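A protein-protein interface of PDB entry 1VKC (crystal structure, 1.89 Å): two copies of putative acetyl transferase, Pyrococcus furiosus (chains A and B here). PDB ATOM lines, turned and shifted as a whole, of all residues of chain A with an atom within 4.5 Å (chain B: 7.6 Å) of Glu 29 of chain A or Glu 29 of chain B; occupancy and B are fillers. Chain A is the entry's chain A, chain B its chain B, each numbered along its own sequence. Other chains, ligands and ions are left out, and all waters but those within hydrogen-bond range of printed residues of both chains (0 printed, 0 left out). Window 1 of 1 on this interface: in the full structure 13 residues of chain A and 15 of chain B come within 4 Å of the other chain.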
ATOM      1  N   LYS A  25      23.460  14.152 -31.027  1.00  0.00           N
ATOM      2  CA  LYS A  25      22.390  13.557 -30.208  1.00  0.00           C
ATOM      3  C   LYS A  25      22.526  13.859 -28.727  1.00  0.00           C
ATOM      4  O   LYS A  25      21.530  14.095 -28.041  1.00  0.00           O
ATOM      5  CB  LYS A  25      22.294  12.054 -30.451  1.00  0.00           C
ATOM      6  CG  LYS A  25      21.622  11.713 -31.775  1.00  0.00           C
ATOM      7  CD  LYS A  25      21.986  10.288 -32.244  1.00  0.00           C
ATOM      8  CE  LYS A  25      21.038   9.804 -33.314  1.00  0.00           C
ATOM      9  N   LEU A  26      23.752  13.880 -28.226  1.00  0.00           N
ATOM     10  CA  LEU A  26      23.979  14.240 -26.840  1.00  0.00           C
ATOM     11  C   LEU A  26      23.636  15.722 -26.587  1.00  0.00           C
ATOM     12  O   LEU A  26      22.988  16.069 -25.590  1.00  0.00           O
ATOM     13  CB  LEU A  26      25.426  13.925 -26.461  1.00  0.00           C
ATOM     14  CG  LEU A  26      25.927  14.267 -25.065  1.00  0.00           C
ATOM     15  CD1 LEU A  26      25.085  13.635 -23.991  1.00  0.00           C
ATOM     16  CD2 LEU A  26      27.383  13.833 -24.956  1.00  0.00           C
ATOM     17  N   ASP A  27      24.051  16.584 -27.501  1.00  0.00           N
ATOM     18  CA  ASP A  27      23.692  17.987 -27.421  1.00  0.00           C
ATOM     19  C   ASP A  27      22.173  18.203 -27.510  1.00  0.00           C
ATOM     20  O   ASP A  27      21.639  19.053 -26.830  1.00  0.00           O
ATOM     21  CB  ASP A  27      24.381  18.770 -28.511  1.00  0.00           C
ATOM     22  CG  ASP A  27      23.996  20.231 -28.499  1.00  0.00           C
ATOM     23  OD1 ASP A  27      24.312  20.944 -27.514  1.00  0.00           O
ATOM     24  OD2 ASP A  27      23.354  20.735 -29.431  1.00  0.00           O
ATOM     25  N   ARG A  28      21.502  17.443 -28.357  1.00  0.00           N
ATOM     26  CA  ARG A  28      20.035  17.489 -28.433  1.00  0.00           C
ATOM     27  C   ARG A  28      19.411  17.150 -27.082  1.00  0.00           C
ATOM     28  O   ARG A  28      18.505  17.833 -26.617  1.00  0.00           O
ATOM     29  CB  ARG A  28      19.535  16.511 -29.481  1.00  0.00           C
ATOM     30  CG  ARG A  28      18.018  16.360 -29.526  1.00  0.00           C
ATOM     31  CD  ARG A  28      17.536  15.704 -30.780  1.00  0.00           C
ATOM     32  NE  ARG A  28      18.063  16.421 -31.940  1.00  0.00           N
ATOM     33  CZ  ARG A  28      18.189  15.919 -33.162  1.00  0.00           C
ATOM     34  NH1 ARG A  28      17.805  14.664 -33.441  1.00  0.00           N
ATOM     35  NH2 ARG A  28      18.714  16.679 -34.122  1.00  0.00           N
ATOM     36  N   GLU A  29      19.909  16.092 -26.457  1.00  0.00           N
ATOM     37  CA  GLU A  29      19.400  15.648 -25.156  1.00  0.00           C
ATOM     38  C   GLU A  29      19.678  16.686 -24.069  1.00  0.00           C
ATOM     39  O   GLU A  29      18.770  17.078 -23.320  1.00  0.00           O
ATOM     40  CB  GLU A  29      20.011  14.272 -24.788  1.00  0.00           C
ATOM     41  CG  GLU A  29      19.541  13.683 -23.443  1.00  0.00           C
ATOM     42  CD  GLU A  29      18.084  13.216 -23.449  1.00  0.00           C
ATOM     43  OE1 GLU A  29      17.390  13.398 -22.425  1.00  0.00           O
ATOM     44  OE2 GLU A  29      17.637  12.655 -24.460  1.00  0.00           O
ATOM     45  N   ILE A  30      20.925  17.128 -23.983  1.00  0.00           N
ATOM     46  CA  ILE A  30      21.330  18.099 -22.978  1.00  0.00           C
ATOM     47  C   ILE A  30      20.582  19.447 -23.134  1.00  0.00           C
ATOM     48  O   ILE A  30      19.991  19.958 -22.165  1.00  0.00           O
ATOM     49  CB  ILE A  30      22.864  18.317 -23.019  1.00  0.00           C
ATOM     50  CG1 ILE A  30      23.589  17.070 -22.478  1.00  0.00           C
ATOM     51  CG2 ILE A  30      23.279  19.544 -22.183  1.00  0.00           C
ATOM     52  CD1 ILE A  30      25.087  17.145 -22.558  1.00  0.00           C
ATOM     53  N   SER A  31      20.599  19.993 -24.354  1.00  0.00           N
ATOM     54  CA  SER A  31      20.090  21.358 -24.611  1.00  0.00           C
ATOM     55  C   SER A  31      18.616  21.513 -24.293  1.00  0.00           C
ATOM     56  O   SER A  31      18.152  22.616 -23.985  1.00  0.00           O
ATOM     57  CB  SER A  31      20.333  21.756 -26.060  1.00  0.00           C
ATOM     58  OG  SER A  31      21.705  21.872 -26.313  1.00  0.00           O
ATOM     59  N   TYR A  32      17.872  20.419 -24.371  1.00  0.00           N
ATOM     60  CA  TYR A  32      16.422  20.496 -24.218  1.00  0.00           C
ATOM     61  C   TYR A  32      15.990  20.998 -22.831  1.00  0.00           C
ATOM     62  O   TYR A  32      14.922  21.592 -22.696  1.00  0.00           O
ATOM     63  CB  TYR A  32      15.763  19.154 -24.533  1.00  0.00           C
ATOM     64  CG  TYR A  32      14.286  19.197 -24.344  1.00  0.00           C
ATOM     65  CD1 TYR A  32      13.496  19.994 -25.151  1.00  0.00           C
ATOM     66  CD2 TYR A  32      13.675  18.479 -23.313  1.00  0.00           C
ATOM     67  CE1 TYR A  32      12.127  20.059 -24.972  1.00  0.00           C
ATOM     68  CE2 TYR A  32      12.307  18.537 -23.120  1.00  0.00           C
ATOM     69  CZ  TYR A  32      11.540  19.329 -23.951  1.00  0.00           C
ATOM     70  OH  TYR A  32      10.191  19.395 -23.765  1.00  0.00           O
ATOM     71  N   SER A  33      16.817  20.786 -21.815  1.00  0.00           N
ATOM     72  CA  SER A  33      16.476  21.244 -20.462  1.00  0.00           C
ATOM     73  C   SER A  33      16.361  22.765 -20.368  1.00  0.00           C
ATOM     74  O   SER A  33      15.602  23.283 -19.548  1.00  0.00           O
ATOM     75  CB  SER A  33      17.496  20.732 -19.437  1.00  0.00           C
ATOM     76  OG  SER A  33      18.776  21.296 -19.659  1.00  0.00           O
ATOM     77  N   TYR A  41       8.270  18.452 -28.229  1.00  0.00           N
ATOM     78  CA  TYR A  41       9.574  17.829 -28.358  1.00  0.00           C
ATOM     79  C   TYR A  41       9.889  17.562 -29.838  1.00  0.00           C
ATOM     80  O   TYR A  41      11.024  17.717 -30.273  1.00  0.00           O
ATOM     81  CB  TYR A  41       9.691  16.551 -27.514  1.00  0.00           C
ATOM     82  CG  TYR A  41      11.097  16.008 -27.550  1.00  0.00           C
ATOM     83  CD1 TYR A  41      12.115  16.636 -26.843  1.00  0.00           C
ATOM     84  CD2 TYR A  41      11.420  14.899 -28.325  1.00  0.00           C
ATOM     85  CE1 TYR A  41      13.420  16.176 -26.904  1.00  0.00           C
ATOM     86  CE2 TYR A  41      12.715  14.424 -28.381  1.00  0.00           C
ATOM     87  CZ  TYR A  41      13.714  15.075 -27.656  1.00  0.00           C
ATOM     88  OH  TYR A  41      14.996  14.623 -27.694  1.00  0.00           O
ATOM     89  N   ILE B  23       5.508   9.676 -29.230  1.00  0.00           N
ATOM     90  CA  ILE B  23       5.474   9.177 -27.858  1.00  0.00           C
ATOM     91  C   ILE B  23       6.821   8.509 -27.502  1.00  0.00           C
ATOM     92  O   ILE B  23       7.367   8.736 -26.419  1.00  0.00           O
ATOM     93  CB  ILE B  23       4.301   8.180 -27.676  1.00  0.00           C
ATOM     94  CG1 ILE B  23       2.967   8.940 -27.650  1.00  0.00           C
ATOM     95  CG2 ILE B  23       4.472   7.356 -26.391  1.00  0.00           C
ATOM     96  CD1 ILE B  23       1.750   8.044 -27.731  1.00  0.00           C
ATOM     97  N   LYS B  24       7.337   7.683 -28.411  1.00  0.00           N
ATOM     98  CA  LYS B  24       8.585   6.953 -28.160  1.00  0.00           C
ATOM     99  C   LYS B  24       9.732   7.936 -27.930  1.00  0.00           C
ATOM    100  O   LYS B  24      10.562   7.780 -27.007  1.00  0.00           O
ATOM    101  CB  LYS B  24       8.893   6.001 -29.331  1.00  0.00           C
ATOM    102  CG  LYS B  24      10.237   5.298 -29.221  1.00  0.00           C
ATOM    103  CD  LYS B  24      10.327   3.985 -30.009  1.00  0.00           C
ATOM    104  CE  LYS B  24      10.394   4.171 -31.493  1.00  0.00           C
ATOM    105  NZ  LYS B  24      10.827   2.861 -32.173  1.00  0.00           N
ATOM    106  N   LYS B  25       9.768   8.963 -28.767  1.00  0.00           N
ATOM    107  CA  LYS B  25      10.822   9.965 -28.702  1.00  0.00           C
ATOM    108  C   LYS B  25      10.714  10.817 -27.443  1.00  0.00           C
ATOM    109  O   LYS B  25      11.735  11.111 -26.813  1.00  0.00           O
ATOM    110  CB  LYS B  25      10.830  10.818 -29.966  1.00  0.00           C
ATOM    111  CG  LYS B  25      11.404  10.046 -31.154  1.00  0.00           C
ATOM    112  CD  LYS B  25      11.490  10.889 -32.431  1.00  0.00           C
ATOM    113  CE  LYS B  25      12.652  10.436 -33.338  1.00  0.00           C
ATOM    114  NZ  LYS B  25      13.973  11.137 -33.023  1.00  0.00           N
ATOM    115  N   LEU B  26       9.496  11.182 -27.056  1.00  0.00           N
ATOM    116  CA  LEU B  26       9.286  11.954 -25.809  1.00  0.00           C
ATOM    117  C   LEU B  26       9.646  11.111 -24.582  1.00  0.00           C
ATOM    118  O   LEU B  26      10.277  11.610 -23.615  1.00  0.00           O
ATOM    119  CB  LEU B  26       7.839  12.466 -25.698  1.00  0.00           C
ATOM    120  CG  LEU B  26       7.528  13.304 -24.439  1.00  0.00           C
ATOM    121  CD1 LEU B  26       8.300  14.599 -24.434  1.00  0.00           C
ATOM    122  CD2 LEU B  26       6.035  13.575 -24.351  1.00  0.00           C
ATOM    123  N   ASP B  27       9.263   9.835 -24.612  1.00  0.00           N
ATOM    124  CA  ASP B  27       9.605   8.931 -23.515  1.00  0.00           C
ATOM    125  C   ASP B  27      11.118   8.796 -23.360  1.00  0.00           C
ATOM    126  O   ASP B  27      11.631   8.771 -22.244  1.00  0.00           O
ATOM    127  CB  ASP B  27       8.965   7.560 -23.724  1.00  0.00           C
ATOM    128  CG  ASP B  27       9.323   6.570 -22.630  1.00  0.00           C
ATOM    129  OD1 ASP B  27       9.007   6.808 -21.433  1.00  0.00           O
ATOM    130  OD2 ASP B  27       9.924   5.514 -22.879  1.00  0.00           O
ATOM    131  N   ARG B  28      11.820   8.702 -24.484  1.00  0.00           N
ATOM    132  CA  ARG B  28      13.268   8.572 -24.505  1.00  0.00           C
ATOM    133  C   ARG B  28      13.908   9.790 -23.853  1.00  0.00           C
ATOM    134  O   ARG B  28      14.887   9.670 -23.093  1.00  0.00           O
ATOM    135  CB  ARG B  28      13.761   8.443 -25.959  1.00  0.00           C
ATOM    136  CG  ARG B  28      15.302   8.304 -26.121  1.00  0.00           C
ATOM    137  CD  ARG B  28      15.769   8.524 -27.540  1.00  0.00           C
ATOM    138  NE  ARG B  28      15.447   9.871 -28.021  1.00  0.00           N
ATOM    139  CZ  ARG B  28      15.340  10.232 -29.308  1.00  0.00           C
ATOM    140  NH1 ARG B  28      15.525   9.352 -30.303  1.00  0.00           N
ATOM    141  NH2 ARG B  28      15.048  11.487 -29.605  1.00  0.00           N
ATOM    142  N   GLU B  29      13.361  10.965 -24.157  1.00  0.00           N
ATOM    143  CA  GLU B  29      13.907  12.215 -23.647  1.00  0.00           C
ATOM    144  C   GLU B  29      13.710  12.277 -22.161  1.00  0.00           C
ATOM    145  O   GLU B  29      14.649  12.536 -21.435  1.00  0.00           O
ATOM    146  CB  GLU B  29      13.221  13.425 -24.301  1.00  0.00           C
ATOM    147  CG  GLU B  29      13.644  14.777 -23.731  1.00  0.00           C
ATOM    148  CD  GLU B  29      15.116  15.096 -23.956  1.00  0.00           C
ATOM    149  OE1 GLU B  29      15.650  14.783 -25.046  1.00  0.00           O
ATOM    150  OE2 GLU B  29      15.735  15.694 -23.051  1.00  0.00           O
ATOM    151  N   ILE B  30      12.477  12.040 -21.730  1.00  0.00           N
ATOM    152  CA  ILE B  30      12.087  12.114 -20.341  1.00  0.00           C
ATOM    153  C   ILE B  30      12.797  11.074 -19.484  1.00  0.00           C
ATOM    154  O   ILE B  30      13.262  11.380 -18.397  1.00  0.00           O
ATOM    155  CB  ILE B  30      10.545  11.955 -20.204  1.00  0.00           C
ATOM    156  CG1 ILE B  30       9.843  13.190 -20.769  1.00  0.00           C
ATOM    157  CG2 ILE B  30      10.125  11.727 -18.721  1.00  0.00           C
ATOM    158  CD1 ILE B  30       8.360  13.054 -20.876  1.00  0.00           C
ATOM    159  N   SER B  31      12.848   9.832 -19.960  1.00  0.00           N
ATOM    160  CA  SER B  31      13.334   8.732 -19.118  1.00  0.00           C
ATOM    161  C   SER B  31      14.828   8.805 -18.790  1.00  0.00           C
ATOM    162  O   SER B  31      15.270   8.258 -17.776  1.00  0.00           O
ATOM    163  CB  SER B  31      13.013   7.388 -19.769  1.00  0.00           C
ATOM    164  OG  SER B  31      11.620   7.237 -19.915  1.00  0.00           O
ATOM    165  N   TYR B  32      15.603   9.459 -19.635  1.00  0.00           N
ATOM    166  CA  TYR B  32      17.046   9.470 -19.468  1.00  0.00           C
ATOM    167  C   TYR B  32      17.520  10.066 -18.130  1.00  0.00           C
ATOM    168  O   TYR B  32      18.541   9.630 -17.568  1.00  0.00           O
ATOM    169  CB  TYR B  32      17.683  10.222 -20.615  1.00  0.00           C
ATOM    170  CG  TYR B  32      19.157  10.229 -20.556  1.00  0.00           C
ATOM    171  CD1 TYR B  32      19.880   9.047 -20.630  1.00  0.00           C
ATOM    172  CD2 TYR B  32      19.851  11.422 -20.420  1.00  0.00           C
ATOM    173  CE1 TYR B  32      21.271   9.056 -20.583  1.00  0.00           C
ATOM    174  CE2 TYR B  32      21.222  11.448 -20.381  1.00  0.00           C
ATOM    175  CZ  TYR B  32      21.932  10.272 -20.459  1.00  0.00           C
ATOM    176  OH  TYR B  32      23.298  10.322 -20.402  1.00  0.00           O
ATOM    177  N   SER B  33      16.780  11.036 -17.616  1.00  0.00           N
ATOM    178  CA  SER B  33      17.183  11.719 -16.385  1.00  0.00           C
ATOM    179  C   SER B  33      17.095  10.801 -15.145  1.00  0.00           C
ATOM    180  O   SER B  33      17.759  11.058 -14.143  1.00  0.00           O
ATOM    181  CB  SER B  33      16.387  13.018 -16.195  1.00  0.00           C
ATOM    182  OG  SER B  33      15.048  12.752 -15.850  1.00  0.00           O
ATOM    183  N   PHE B  34      16.325   9.710 -15.242  1.00  0.00           N
ATOM    184  CA  PHE B  34      16.187   8.753 -14.145  1.00  0.00           C
ATOM    185  C   PHE B  34      17.147   7.545 -14.185  1.00  0.00           C
ATOM    186  O   PHE B  34      17.097   6.699 -13.318  1.00  0.00           O
ATOM    187  CB  PHE B  34      14.751   8.251 -14.090  1.00  0.00           C
ATOM    188  CG  PHE B  34      13.747   9.345 -13.932  1.00  0.00           C
ATOM    189  CD1 PHE B  34      12.981   9.768 -15.012  1.00  0.00           C
ATOM    190  CD2 PHE B  34      13.588   9.979 -12.712  1.00  0.00           C
ATOM    191  CE1 PHE B  34      12.053  10.795 -14.864  1.00  0.00           C
ATOM    192  CE2 PHE B  34      12.670  11.002 -12.557  1.00  0.00           C
ATOM    193  CZ  PHE B  34      11.897  11.410 -13.636  1.00  0.00           C
ATOM    194  N   TYR B  41      24.957   7.831 -23.830  1.00  0.00           N
ATOM    195  CA  TYR B  41      23.667   8.200 -24.370  1.00  0.00           C
ATOM    196  C   TYR B  41      23.345   7.330 -25.584  1.00  0.00           C
ATOM    197  O   TYR B  41      22.186   6.960 -25.818  1.00  0.00           O
ATOM    198  CB  TYR B  41      23.599   9.689 -24.738  1.00  0.00           C
ATOM    199  CG  TYR B  41      22.205  10.043 -25.141  1.00  0.00           C
ATOM    200  CD1 TYR B  41      21.858  10.179 -26.476  1.00  0.00           C
ATOM    201  CD2 TYR B  41      21.201  10.146 -24.183  1.00  0.00           C
ATOM    202  CE1 TYR B  41      20.550  10.460 -26.847  1.00  0.00           C
ATOM    203  CE2 TYR B  41      19.886  10.424 -24.543  1.00  0.00           C
ATOM    204  CZ  TYR B  41      19.569  10.578 -25.868  1.00  0.00           C
ATOM    205  OH  TYR B  41      18.268  10.864 -26.220  1.00  0.00           O
ATOM    206  N   TYR B  44      22.169   4.099 -24.195  1.00  0.00           N
ATOM    207  CA  TYR B  44      20.816   4.339 -23.695  1.00  0.00           C
ATOM    208  C   TYR B  44      19.792   4.348 -24.844  1.00  0.00           C
ATOM    209  O   TYR B  44      18.730   3.696 -24.764  1.00  0.00           O
ATOM    210  CB  TYR B  44      20.746   5.648 -22.899  1.00  0.00           C
ATOM    211  CG  TYR B  44      19.338   6.118 -22.669  1.00  0.00           C
ATOM    212  CD1 TYR B  44      18.802   7.177 -23.404  1.00  0.00           C
ATOM    213  CD2 TYR B  44      18.529   5.495 -21.740  1.00  0.00           C
ATOM    214  CE1 TYR B  44      17.487   7.611 -23.190  1.00  0.00           C
ATOM    215  CE2 TYR B  44      17.223   5.917 -21.531  1.00  0.00           C
ATOM    216  CZ  TYR B  44      16.711   6.970 -22.258  1.00  0.00           C
ATOM    217  OH  TYR B  44      15.425   7.378 -22.037  1.00  0.00           O
ATOM    218  N   GLU B  45      20.081   5.097 -25.906  1.00  0.00           N
ATOM    219  CA  GLU B  45      19.157   5.169 -27.041  1.00  0.00           C
ATOM    220  C   GLU B  45      18.802   3.816 -27.596  1.00  0.00           C
ATOM    221  O   GLU B  45      17.625   3.544 -27.897  1.00  0.00           O
ATOM    222  CB  GLU B  45      19.725   6.009 -28.185  1.00  0.00           C
ATOM    223  CG  GLU B  45      19.611   7.508 -27.969  1.00  0.00           C
ATOM    224  CD  GLU B  45      19.238   8.265 -29.245  1.00  0.00           C
ATOM    225  OE1 GLU B  45      19.731   7.902 -30.333  1.00  0.00           O
ATOM    226  OE2 GLU B  45      18.439   9.214 -29.152  1.00  0.00           O
ATOM    227  N   HIS B  48      16.769   1.792 -24.967  1.00  0.00           N
ATOM    228  CA  HIS B  48      15.435   2.353 -24.894  1.00  0.00           C
ATOM    229  C   HIS B  48      14.585   1.905 -26.077  1.00  0.00           C
ATOM    230  O   HIS B  48      13.449   1.515 -25.892  1.00  0.00           O
ATOM    231  CB  HIS B  48      15.447   3.877 -24.866  1.00  0.00           C
ATOM    232  CG  HIS B  48      14.071   4.456 -24.849  1.00  0.00           C
ATOM    233  ND1 HIS B  48      13.383   4.771 -25.998  1.00  0.00           N
ATOM    234  CD2 HIS B  48      13.223   4.688 -23.828  1.00  0.00           C
ATOM    235  CE1 HIS B  48      12.185   5.215 -25.675  1.00  0.00           C
ATOM    236  NE2 HIS B  48      12.066   5.176 -24.364  1.00  0.00           N
ATOM    237  N   GLU B  98       2.926  10.348 -19.287  1.00  0.00           N
ATOM    238  CA  GLU B  98       3.930  11.408 -19.416  1.00  0.00           C
ATOM    239  C   GLU B  98       3.282  12.661 -19.977  1.00  0.00           C
ATOM    240  O   GLU B  98       2.439  12.584 -20.872  1.00  0.00           O
ATOM    241  CB  GLU B  98       5.081  10.938 -20.314  1.00  0.00           C
ATOM    242  CG  GLU B  98       6.000   9.918 -19.633  1.00  0.00           C
ATOM    243  CD  GLU B  98       6.979   9.215 -20.579  1.00  0.00           C
ATOM    244  OE1 GLU B  98       8.022   8.702 -20.088  1.00  0.00           O
ATOM    245  OE2 GLU B  98       6.714   9.168 -21.794  1.00  0.00           O
ATOM    246  N   LYS B 101       6.756  19.063 -20.260  1.00  0.00           N
ATOM    247  CA  LYS B 101       7.126  19.765 -19.036  1.00  0.00           C
ATOM    248  C   LYS B 101       6.354  21.066 -18.872  1.00  0.00           C
ATOM    249  O   LYS B 101       5.942  21.407 -17.765  1.00  0.00           O
ATOM    250  CB  LYS B 101       8.635  20.014 -18.974  1.00  0.00           C
ATOM    251  CG  LYS B 101       9.197  20.885 -20.101  1.00  0.00           C
ATOM    252  CD  LYS B 101      10.687  20.990 -19.982  1.00  0.00           C
ATOM    253  CE  LYS B 101      11.284  21.730 -21.161  1.00  0.00           C
ATOM    254  NZ  LYS B 101      12.756  21.807 -21.030  1.00  0.00           N
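CE1 of Tyr 41 of chain B touches O of Lys 25 of chain A, 3.9 Å away. Lys 25 of chain A touches Glu 45 of chain B. Glu 29 of chain A touches Tyr 32 of chain B. Glu 29 of chain B touches Tyr 32 of chain A. Lys 101 of chain B touches Ser 33 of chain A (NZ to O, 3.5 Å). O of Lys 25 of chain B touches CE2 of Tyr 41 of chain A, 3.8 Å away. Tyr 41 of chain A touches Leu 26 of chain B. OH of Tyr 41 of chain A touches NH2 of Arg 28 of chain B, at 3.7 Å.
The backbone carbonyl oxygen (O) of Arg 28 of chain B sits at hydrogen-bond distance from the side-chain hydroxyl (OH) of Tyr 44 of chain B, at 2.6 Å. NH1 of Arg 28 of chain B lies within salt-bridge range of OE2 of Glu 45 of chain B (3.1 Å). The side-chain hydroxyl of Tyr 44 of chain B sits at hydrogen-bond distance from the backbone NH of Tyr 32 of chain B, 3.2 Å away. NE of Arg 28 of chain B is in hydrogen-bond range of OH of Tyr 41 of chain B, at 3.5 Å. The backbone carbonyl oxygen (O) of Ile 30 of chain A lies within hydrogen-bond range of the side-chain hydroxyl (OG) of Ser 33 of chain A (3.1 Å). The side-chain carboxylate (OE2) of Glu 45 of chain B lies close to the side-chain hydroxyl (OH) of Tyr 41 of chain B (3.4 Å).
The backbone carbonyl oxygen (O) of Tyr 32 of chain A sits at hydrogen-bond distance from the side-chain amino group (NZ) of Lys 101 of chain B, at 2.7 Å. OE1 of Glu 29 of chain A sits close to OE2 of Glu 29 of chain B (2.9 Å). The side-chain carboxylate (OE2) of Glu 29 of chain A sits at hydrogen-bond distance from the side-chain hydroxyl (OH) of Tyr 41 of chain B (2.6 Å). OE1 of Glu 29 of chain B is in hydrogen-bond range of OH of Tyr 41 of chain A (2.7 Å).
Of the 18 printed residues of chain B, 8 touch a printed residue of chain A. Of the 10 printed residues of chain A, 5 touch a printed residue of chain B. Printed residues of chain A that touch a printed residue of chain B: Lys 25, Glu 29, Tyr 32, Ser 33 and Tyr 41. Among the printed residues, no Asp or Glu carboxylate lies within 4 Å of a Lys or Arg side-chain nitrogen of the other chain.
Of chain B, only Glu 29 (2.9 Å), Tyr 32 (3.7 Å) and Tyr 41 (2.6 Å) come within 4 Å of Glu 29 of chain A. Of chain A, only Glu 29, Tyr 32 and Tyr 41 come within 4 Å of Glu 29 of chain B. Printed residues of chain A within 4 Å of Tyr 32 of chain B: Glu 29 (3.7 Å). Of the printed residues of chain A, Leu 26 of chain B touches Tyr 41 (3.9 Å). Of the printed residues of chain A, Arg 28 of chain B touches Tyr 41. Of the printed residues of chain B, Tyr 32 of chain A touches Glu 29 (3.5 Å) and Lys 101 (2.7 Å). Ile 30 of chain B touches none of the printed residues of chain A. Glu 98 of chain B touches none of the printed residues of chain A. The nearest printed residue of chain A that does not touch Glu 29 of chain B is Arg 28 of chain A (4.5 Å).
Glu 29 of chain A touches its own counterpart, Glu 29 of chain B. Glu 29 of chain A touches Tyr 41 of chain B, and with the chains exchanged Tyr 41 of chain A touches Glu 29 of chain B. Tyr 41 of chain A touches Leu 26 of chain B, but with the chains exchanged Leu 26 of chain A does not touch Tyr 41 of chain B (4.3 Å). Tyr 41 of chain A touches Arg 28 of chain B, but with the chains exchanged Arg 28 of chain A does not touch Tyr 41 of chain B (6.4 Å).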
